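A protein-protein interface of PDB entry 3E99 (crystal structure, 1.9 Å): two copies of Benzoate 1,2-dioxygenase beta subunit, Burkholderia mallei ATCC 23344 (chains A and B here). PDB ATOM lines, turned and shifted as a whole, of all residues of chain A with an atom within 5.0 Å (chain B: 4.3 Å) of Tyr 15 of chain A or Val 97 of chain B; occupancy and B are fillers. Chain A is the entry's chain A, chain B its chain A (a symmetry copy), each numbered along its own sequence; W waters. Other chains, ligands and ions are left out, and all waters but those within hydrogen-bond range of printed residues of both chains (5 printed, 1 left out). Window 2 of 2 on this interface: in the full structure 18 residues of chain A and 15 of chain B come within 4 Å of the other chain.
Water W5 lies within hydrogen-bond range of the backbone carbonyl oxygen (O) of Ile 94 of chain A (2.6 Å), the backbone NH (N) of Asn 96 of chain B (2.9 Å) and the side-chain hydroxyl (OH) of Tyr 15 of chain A (3.3 Å). Water W2 lies within hydrogen-bond range of the side-chain carboxylate (OE1) of Glu 98 of chain B (2.7 Å) and the backbone carbonyl oxygen (O) of Ala 12 of chain A (2.7 Å). Water W4 lies within hydrogen-bond range of the backbone carbonyl oxygen (O) of Tyr 15 of chain A (2.7 Å), the side-chain amide nitrogen (ND2) of Asn 96 of chain B (2.9 Å), the side-chain hydroxyl (OG) of Ser 18 of chain A (3.4 Å) and the backbone NH (N) of Arg 19 of chain A (3.5 Å). Water W3 bridges OH of Tyr 15 of chain A (2.7 Å) and NE2 of Gln 11 of chain B (2.8 Å). Water W1 bridges OE1 of Glu 98 of chain B (3.3 Å) and NH2 of Arg 19 of chain A (3.5 Å).
Among the printed residues, pairs that only touch across the chains: Arg 19 of chain A with Arg 110 of chain B (3.3 Å), Tyr 15 of chain A with Val 97 of chain B (3.4 Å), Tyr 15 of chain A with Asn 96 of chain B (3.5 Å) and Tyr 15 of chain A with Glu 98 of chain B (3.8 Å).
ND2 of Asn 96 of chain B sits at hydrogen-bond distance from OG of Ser 18 of chain A (3.3 Å). The guanidinium group (NE) of Arg 19 of chain A lies within salt-bridge range of the side-chain carboxylate (OE2) of Glu 98 of chain B (2.9 Å). OD1 of Asn 96 of chain B lies within hydrogen-bond range of N of Ile 94 of chain A, at 2.9 Å.
O of Leu 14 of chain A is in hydrogen-bond range of OG of Ser 18 of chain A. The backbone carbonyl oxygen (O) of Tyr 15 of chain A is in hydrogen-bond range of the side-chain hydroxyl (OG) of Ser 18 of chain A (3.2 Å). The backbone carbonyl oxygen (O) of Glu 98 of chain B lies within hydrogen-bond range of the backbone NH (N) of Arg 110 of chain B, at 2.9 Å.
Of the 10 printed residues of chain B, 4 touch a printed residue of chain A. Along chain B the printed residues that touch a printed residue of chain A span positions 96 to 110. Among the printed residues, 7 pairs touch across the chains. Among the printed residues, Asp or Glu carboxylates within 4 Å of a Lys or Arg side-chain nitrogen of the other chain: Arg 19 of chain A with Glu 98 of chain B (2.9 Å).
3 positions are printed for both chains. Of the 7 pairs that touch across the chains among the printed residues, none has its exchanged pair printed and touching as well.
Tyr 15 of chain A touches just these residues of chain B: Asn 96, Val 97 and Glu 98. Of chain A, only Tyr 15 (3.4 Å) comes within 4 Å of Val 97 of chain B. Of the printed residues of chain A, Asn 96 of chain B touches Tyr 15, Ser 18 and Ile 94. Printed residues of chain B within 4 Å of Ser 18 of chain A: Asn 96. Printed residues of chain A within 4 Å of Glu 98 of chain B: Tyr 15 (3.8 Å) and Arg 19 (2.9 Å). Ile 94 of chain B touches none of the printed residues of chain A. The nearest printed residue of chain B that does not touch Tyr 15 of chain A is Gln 11 of chain B (5.0 Å). The nearest printed residue of chain A that does not touch Arg 110 of chain B is Tyr 15 of chain A (7.0 Å).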
ATOM      1  N   GLN A  11       9.245 -13.483  -6.209  1.00  0.00           N
ATOM      2  CA  GLN A  11       9.778 -14.050  -7.443  1.00  0.00           C
ATOM      3  C   GLN A  11       8.757 -14.987  -8.113  1.00  0.00           C
ATOM      4  O   GLN A  11       8.539 -14.939  -9.332  1.00  0.00           O
ATOM      5  CB  GLN A  11      11.135 -14.743  -7.169  1.00  0.00           C
ATOM      6  CG  GLN A  11      12.264 -13.738  -6.935  1.00  0.00           C
ATOM      7  CD  GLN A  11      13.582 -14.367  -6.513  1.00  0.00           C
ATOM      8  OE1 GLN A  11      13.616 -15.242  -5.663  1.00  0.00           O
ATOM      9  NE2 GLN A  11      14.671 -13.898  -7.089  1.00  0.00           N
ATOM     10  N   ALA A  12       8.060 -15.777  -7.311  1.00  0.00           N
ATOM     11  CA  ALA A  12       7.082 -16.711  -7.839  1.00  0.00           C
ATOM     12  C   ALA A  12       6.021 -15.938  -8.592  1.00  0.00           C
ATOM     13  O   ALA A  12       5.615 -16.311  -9.700  1.00  0.00           O
ATOM     14  CB  ALA A  12       6.465 -17.566  -6.707  1.00  0.00           C
ATOM     15  N   PHE A  13       5.584 -14.833  -7.998  1.00  0.00           N
ATOM     16  CA  PHE A  13       4.618 -13.965  -8.620  1.00  0.00           C
ATOM     17  C   PHE A  13       5.110 -13.295  -9.894  1.00  0.00           C
ATOM     18  O   PHE A  13       4.384 -13.269 -10.925  1.00  0.00           O
ATOM     19  CB  PHE A  13       4.177 -12.892  -7.673  1.00  0.00           C
ATOM     20  CG  PHE A  13       3.227 -11.935  -8.295  1.00  0.00           C
ATOM     21  CD1 PHE A  13       1.967 -12.356  -8.667  1.00  0.00           C
ATOM     22  CD2 PHE A  13       3.613 -10.625  -8.562  1.00  0.00           C
ATOM     23  CE1 PHE A  13       1.101 -11.487  -9.255  1.00  0.00           C
ATOM     24  CE2 PHE A  13       2.754  -9.766  -9.166  1.00  0.00           C
ATOM     25  CZ  PHE A  13       1.505 -10.194  -9.530  1.00  0.00           C
ATOM     26  N   LEU A  14       6.329 -12.761  -9.849  1.00  0.00           N
ATOM     27  CA  LEU A  14       6.943 -12.167 -11.024  1.00  0.00           C
ATOM     28  C   LEU A  14       7.065 -13.191 -12.179  1.00  0.00           C
ATOM     29  O   LEU A  14       6.871 -12.840 -13.345  1.00  0.00           O
ATOM     30  CB  LEU A  14       8.322 -11.544 -10.715  1.00  0.00           C
ATOM     31  CG  LEU A  14       8.452 -10.368  -9.727  1.00  0.00           C
ATOM     32  CD1 LEU A  14       9.923  -9.950  -9.496  1.00  0.00           C
ATOM     33  CD2 LEU A  14       7.582  -9.188 -10.246  1.00  0.00           C
ATOM     34  N   TYR A  15       7.414 -14.439 -11.853  1.00  0.00           N
ATOM     35  CA  TYR A  15       7.568 -15.445 -12.873  1.00  0.00           C
ATOM     36  C   TYR A  15       6.200 -15.755 -13.477  1.00  0.00           C
ATOM     37  O   TYR A  15       6.088 -15.905 -14.664  1.00  0.00           O
ATOM     38  CB  TYR A  15       8.227 -16.720 -12.340  1.00  0.00           C
ATOM     39  CG  TYR A  15       9.618 -16.498 -11.717  1.00  0.00           C
ATOM     40  CD1 TYR A  15      10.355 -15.326 -11.945  1.00  0.00           C
ATOM     41  CD2 TYR A  15      10.154 -17.434 -10.876  1.00  0.00           C
ATOM     42  CE1 TYR A  15      11.608 -15.131 -11.398  1.00  0.00           C
ATOM     43  CE2 TYR A  15      11.400 -17.255 -10.291  1.00  0.00           C
ATOM     44  CZ  TYR A  15      12.122 -16.096 -10.551  1.00  0.00           C
ATOM     45  OH  TYR A  15      13.344 -15.958  -9.944  1.00  0.00           O
ATOM     46  N   ARG A  16       5.166 -15.868 -12.638  1.00  0.00           N
ATOM     47  CA  ARG A  16       3.828 -16.155 -13.128  1.00  0.00           C
ATOM     48  C   ARG A  16       3.314 -15.022 -14.012  1.00  0.00           C
ATOM     49  O   ARG A  16       2.825 -15.265 -15.110  1.00  0.00           O
ATOM     50  CB  ARG A  16       2.850 -16.364 -11.958  1.00  0.00           C
ATOM     51  CG  ARG A  16       1.428 -16.541 -12.429  1.00  0.00           C
ATOM     52  CD  ARG A  16       0.510 -17.236 -11.429  1.00  0.00           C
ATOM     53  NE  ARG A  16      -0.736 -17.520 -12.139  1.00  0.00           N
ATOM     54  CZ  ARG A  16      -1.802 -16.735 -12.163  1.00  0.00           C
ATOM     55  NH1 ARG A  16      -1.856 -15.615 -11.443  1.00  0.00           N
ATOM     56  NH2 ARG A  16      -2.835 -17.097 -12.892  1.00  0.00           N
ATOM     57  N   GLU A  17       3.410 -13.785 -13.514  1.00  0.00           N
ATOM     58  CA  GLU A  17       2.930 -12.632 -14.270  1.00  0.00           C
ATOM     59  C   GLU A  17       3.526 -12.575 -15.670  1.00  0.00           C
ATOM     60  O   GLU A  17       2.808 -12.458 -16.664  1.00  0.00           O
ATOM     61  CB  GLU A  17       3.139 -11.344 -13.493  1.00  0.00           C
ATOM     62  CG  GLU A  17       2.577 -10.091 -14.163  1.00  0.00           C
ATOM     63  CD  GLU A  17       3.634  -9.173 -14.727  1.00  0.00           C
ATOM     64  OE1 GLU A  17       4.740  -9.061 -14.142  1.00  0.00           O
ATOM     65  OE2 GLU A  17       3.383  -8.570 -15.792  1.00  0.00           O
ATOM     66  N   SER A  18       4.834 -12.720 -15.754  1.00  0.00           N
ATOM     67  CA  SER A  18       5.529 -12.700 -17.044  1.00  0.00           C
ATOM     68  C   SER A  18       5.210 -13.935 -17.902  1.00  0.00           C
ATOM     69  O   SER A  18       5.102 -13.816 -19.130  1.00  0.00           O
ATOM     70  CB  SER A  18       7.051 -12.470 -16.851  1.00  0.00           C
ATOM     71  OG  SER A  18       7.603 -13.453 -16.026  1.00  0.00           O
ATOM     72  N   ARG A  19       5.019 -15.103 -17.282  1.00  0.00           N
ATOM     73  CA  ARG A  19       4.569 -16.291 -17.995  1.00  0.00           C
ATOM     74  C   ARG A  19       3.217 -16.079 -18.674  1.00  0.00           C
ATOM     75  O   ARG A  19       2.981 -16.555 -19.807  1.00  0.00           O
ATOM     76  CB  ARG A  19       4.482 -17.528 -17.074  1.00  0.00           C
ATOM     77  CG  ARG A  19       3.856 -18.753 -17.738  1.00  0.00           C
ATOM     78  CD  ARG A  19       4.087 -19.993 -16.943  1.00  0.00           C
ATOM     79  NE  ARG A  19       3.787 -19.829 -15.539  1.00  0.00           N
ATOM     80  CZ  ARG A  19       2.572 -19.820 -15.006  1.00  0.00           C
ATOM     81  NH1 ARG A  19       1.500 -19.953 -15.753  1.00  0.00           N
ATOM     82  NH2 ARG A  19       2.430 -19.725 -13.699  1.00  0.00           N
ATOM     83  N   ILE A  94      13.658 -12.651 -15.779  1.00  0.00           N
ATOM     84  CA  ILE A  94      13.631 -11.687 -14.666  1.00  0.00           C
ATOM     85  C   ILE A  94      14.846 -12.006 -13.823  1.00  0.00           C
ATOM     86  O   ILE A  94      14.992 -13.158 -13.370  1.00  0.00           O
ATOM     87  CB  ILE A  94      12.347 -11.858 -13.818  1.00  0.00           C
ATOM     88  CG1 ILE A  94      11.035 -11.676 -14.643  1.00  0.00           C
ATOM     89  CG2 ILE A  94      12.370 -10.942 -12.527  1.00  0.00           C
ATOM     90  CD1 ILE A  94      10.949 -10.408 -15.334  1.00  0.00           C
ATOM     91  N   LEU B   7      12.796 -25.184  -3.782  1.00  0.00           N
ATOM     92  CA  LEU B   7      13.145 -24.578  -5.050  1.00  0.00           C
ATOM     93  C   LEU B   7      14.623 -24.338  -5.157  1.00  0.00           C
ATOM     94  O   LEU B   7      15.201 -24.534  -6.225  1.00  0.00           O
ATOM     95  CB  LEU B   7      12.376 -23.264  -5.239  1.00  0.00           C
ATOM     96  CG  LEU B   7      12.646 -22.510  -6.513  1.00  0.00           C
ATOM     97  CD1 LEU B   7      12.281 -23.379  -7.728  1.00  0.00           C
ATOM     98  CD2 LEU B   7      11.867 -21.168  -6.494  1.00  0.00           C
ATOM     99  N   GLN B  11      17.044 -25.578  -8.072  1.00  0.00           N
ATOM    100  CA  GLN B  11      17.869 -24.618  -8.797  1.00  0.00           C
ATOM    101  C   GLN B  11      19.353 -25.030  -8.774  1.00  0.00           C
ATOM    102  O   GLN B  11      20.051 -24.986  -9.797  1.00  0.00           O
ATOM    103  CB  GLN B  11      17.637 -23.191  -8.244  1.00  0.00           C
ATOM    104  CG  GLN B  11      16.285 -22.617  -8.670  1.00  0.00           C
ATOM    105  CD  GLN B  11      15.946 -21.280  -8.028  1.00  0.00           C
ATOM    106  OE1 GLN B  11      16.125 -21.093  -6.836  1.00  0.00           O
ATOM    107  NE2 GLN B  11      15.427 -20.362  -8.819  1.00  0.00           N
ATOM    108  N   LEU B  14      19.699 -27.700 -11.347  1.00  0.00           N
ATOM    109  CA  LEU B  14      19.612 -27.129 -12.679  1.00  0.00           C
ATOM    110  C   LEU B  14      20.911 -26.378 -13.061  1.00  0.00           C
ATOM    111  O   LEU B  14      21.349 -26.439 -14.212  1.00  0.00           O
ATOM    112  CB  LEU B  14      18.389 -26.198 -12.839  1.00  0.00           C
ATOM    113  CG  LEU B  14      16.956 -26.746 -12.692  1.00  0.00           C
ATOM    114  CD1 LEU B  14      15.886 -25.636 -12.805  1.00  0.00           C
ATOM    115  CD2 LEU B  14      16.748 -27.872 -13.743  1.00  0.00           C
ATOM    116  N   ILE B  94      19.506 -19.903 -16.644  1.00  0.00           N
ATOM    117  CA  ILE B  94      18.232 -20.537 -16.267  1.00  0.00           C
ATOM    118  C   ILE B  94      17.491 -19.503 -15.448  1.00  0.00           C
ATOM    119  O   ILE B  94      18.031 -19.023 -14.433  1.00  0.00           O
ATOM    120  CB  ILE B  94      18.476 -21.803 -15.411  1.00  0.00           C
ATOM    121  CG1 ILE B  94      19.350 -22.876 -16.133  1.00  0.00           C
ATOM    122  CG2 ILE B  94      17.121 -22.412 -14.862  1.00  0.00           C
ATOM    123  CD1 ILE B  94      18.823 -23.296 -17.413  1.00  0.00           C
ATOM    124  N   ALA B  95      16.251 -19.200 -15.852  1.00  0.00           N
ATOM    125  CA  ALA B  95      15.468 -18.081 -15.293  1.00  0.00           C
ATOM    126  C   ALA B  95      14.028 -18.517 -15.014  1.00  0.00           C
ATOM    127  O   ALA B  95      13.488 -19.443 -15.618  1.00  0.00           O
ATOM    128  CB  ALA B  95      15.443 -16.901 -16.300  1.00  0.00           C
ATOM    129  N   ASN B  96      13.405 -17.817 -14.099  1.00  0.00           N
ATOM    130  CA  ASN B  96      11.961 -17.877 -13.908  1.00  0.00           C
ATOM    131  C   ASN B  96      11.511 -19.296 -13.578  1.00  0.00           C
ATOM    132  O   ASN B  96      10.528 -19.822 -14.111  1.00  0.00           O
ATOM    133  CB  ASN B  96      11.212 -17.331 -15.146  1.00  0.00           C
ATOM    134  CG  ASN B  96      11.395 -15.825 -15.380  1.00  0.00           C
ATOM    135  OD1 ASN B  96      12.450 -15.241 -15.147  1.00  0.00           O
ATOM    136  ND2 ASN B  96      10.350 -15.201 -15.927  1.00  0.00           N
ATOM    137  N   VAL B  97      12.245 -19.907 -12.675  1.00  0.00           N
ATOM    138  CA  VAL B  97      11.978 -21.291 -12.291  1.00  0.00           C
ATOM    139  C   VAL B  97      10.728 -21.368 -11.390  1.00  0.00           C
ATOM    140  O   VAL B  97      10.661 -20.714 -10.380  1.00  0.00           O
ATOM    141  CB  VAL B  97      13.145 -21.944 -11.566  1.00  0.00           C
ATOM    142  CG1 VAL B  97      12.775 -23.433 -11.267  1.00  0.00           C
ATOM    143  CG2 VAL B  97      14.465 -21.843 -12.406  1.00  0.00           C
ATOM    144  N   GLU B  98       9.767 -22.183 -11.805  1.00  0.00           N
ATOM    145  CA  GLU B  98       8.545 -22.429 -11.071  1.00  0.00           C
ATOM    146  C   GLU B  98       8.344 -23.893 -10.827  1.00  0.00           C
ATOM    147  O   GLU B  98       8.398 -24.687 -11.757  1.00  0.00           O
ATOM    148  CB  GLU B  98       7.362 -21.947 -11.860  1.00  0.00           C
ATOM    149  CG  GLU B  98       7.356 -20.411 -12.045  1.00  0.00           C
ATOM    150  CD  GLU B  98       6.171 -20.011 -12.844  1.00  0.00           C
ATOM    151  OE1 GLU B  98       5.060 -19.951 -12.273  1.00  0.00           O
ATOM    152  OE2 GLU B  98       6.325 -19.852 -14.048  1.00  0.00           O
ATOM    153  N   ARG B 110       9.145 -25.928 -14.230  1.00  0.00           N
ATOM    154  CA  ARG B 110       9.339 -25.311 -15.545  1.00  0.00           C
ATOM    155  C   ARG B 110      10.222 -24.108 -15.400  1.00  0.00           C
ATOM    156  O   ARG B 110      10.328 -23.511 -14.304  1.00  0.00           O
ATOM    157  CB  ARG B 110       8.023 -24.894 -16.166  1.00  0.00           C
ATOM    158  CG  ARG B 110       7.329 -23.761 -15.480  1.00  0.00           C
ATOM    159  CD  ARG B 110       6.113 -23.346 -16.189  1.00  0.00           C
ATOM    160  NE  ARG B 110       6.365 -22.632 -17.427  1.00  0.00           N
ATOM    161  CZ  ARG B 110       5.491 -22.561 -18.424  1.00  0.00           C
ATOM    162  NH1 ARG B 110       4.304 -23.160 -18.350  1.00  0.00           N
ATOM    163  NH2 ARG B 110       5.778 -21.842 -19.493  1.00  0.00           N
ATOM    164  N   PHE B 111      10.852 -23.703 -16.497  1.00  0.00           N
ATOM    165  CA  PHE B 111      11.769 -22.562 -16.426  1.00  0.00           C
ATOM    166  C   PHE B 111      12.035 -22.019 -17.826  1.00  0.00           C
ATOM    167  O   PHE B 111      11.806 -22.721 -18.817  1.00  0.00           O
ATOM    168  CB  PHE B 111      13.106 -22.876 -15.655  1.00  0.00           C
ATOM    169  CG  PHE B 111      13.938 -23.985 -16.246  1.00  0.00           C
ATOM    170  CD1 PHE B 111      14.831 -23.752 -17.300  1.00  0.00           C
ATOM    171  CD2 PHE B 111      13.762 -25.276 -15.831  1.00  0.00           C
ATOM    172  CE1 PHE B 111      15.542 -24.760 -17.844  1.00  0.00           C
ATOM    173  CE2 PHE B 111      14.459 -26.293 -16.399  1.00  0.00           C
ATOM    174  CZ  PHE B 111      15.366 -26.047 -17.406  1.00  0.00           C
HETATM  175  O   HOH W   1       3.403 -22.761 -12.281  1.00  0.00           O
HETATM  176  O   HOH W   2       4.789 -18.904  -9.803  1.00  0.00           O
HETATM  177  O   HOH W   3      14.440 -17.776  -8.202  1.00  0.00           O
HETATM  178  O   HOH W   4       7.936 -16.809 -16.451  1.00  0.00           O
HETATM  179  O   HOH W   5      14.980 -15.710 -12.828  1.00  0.00           O
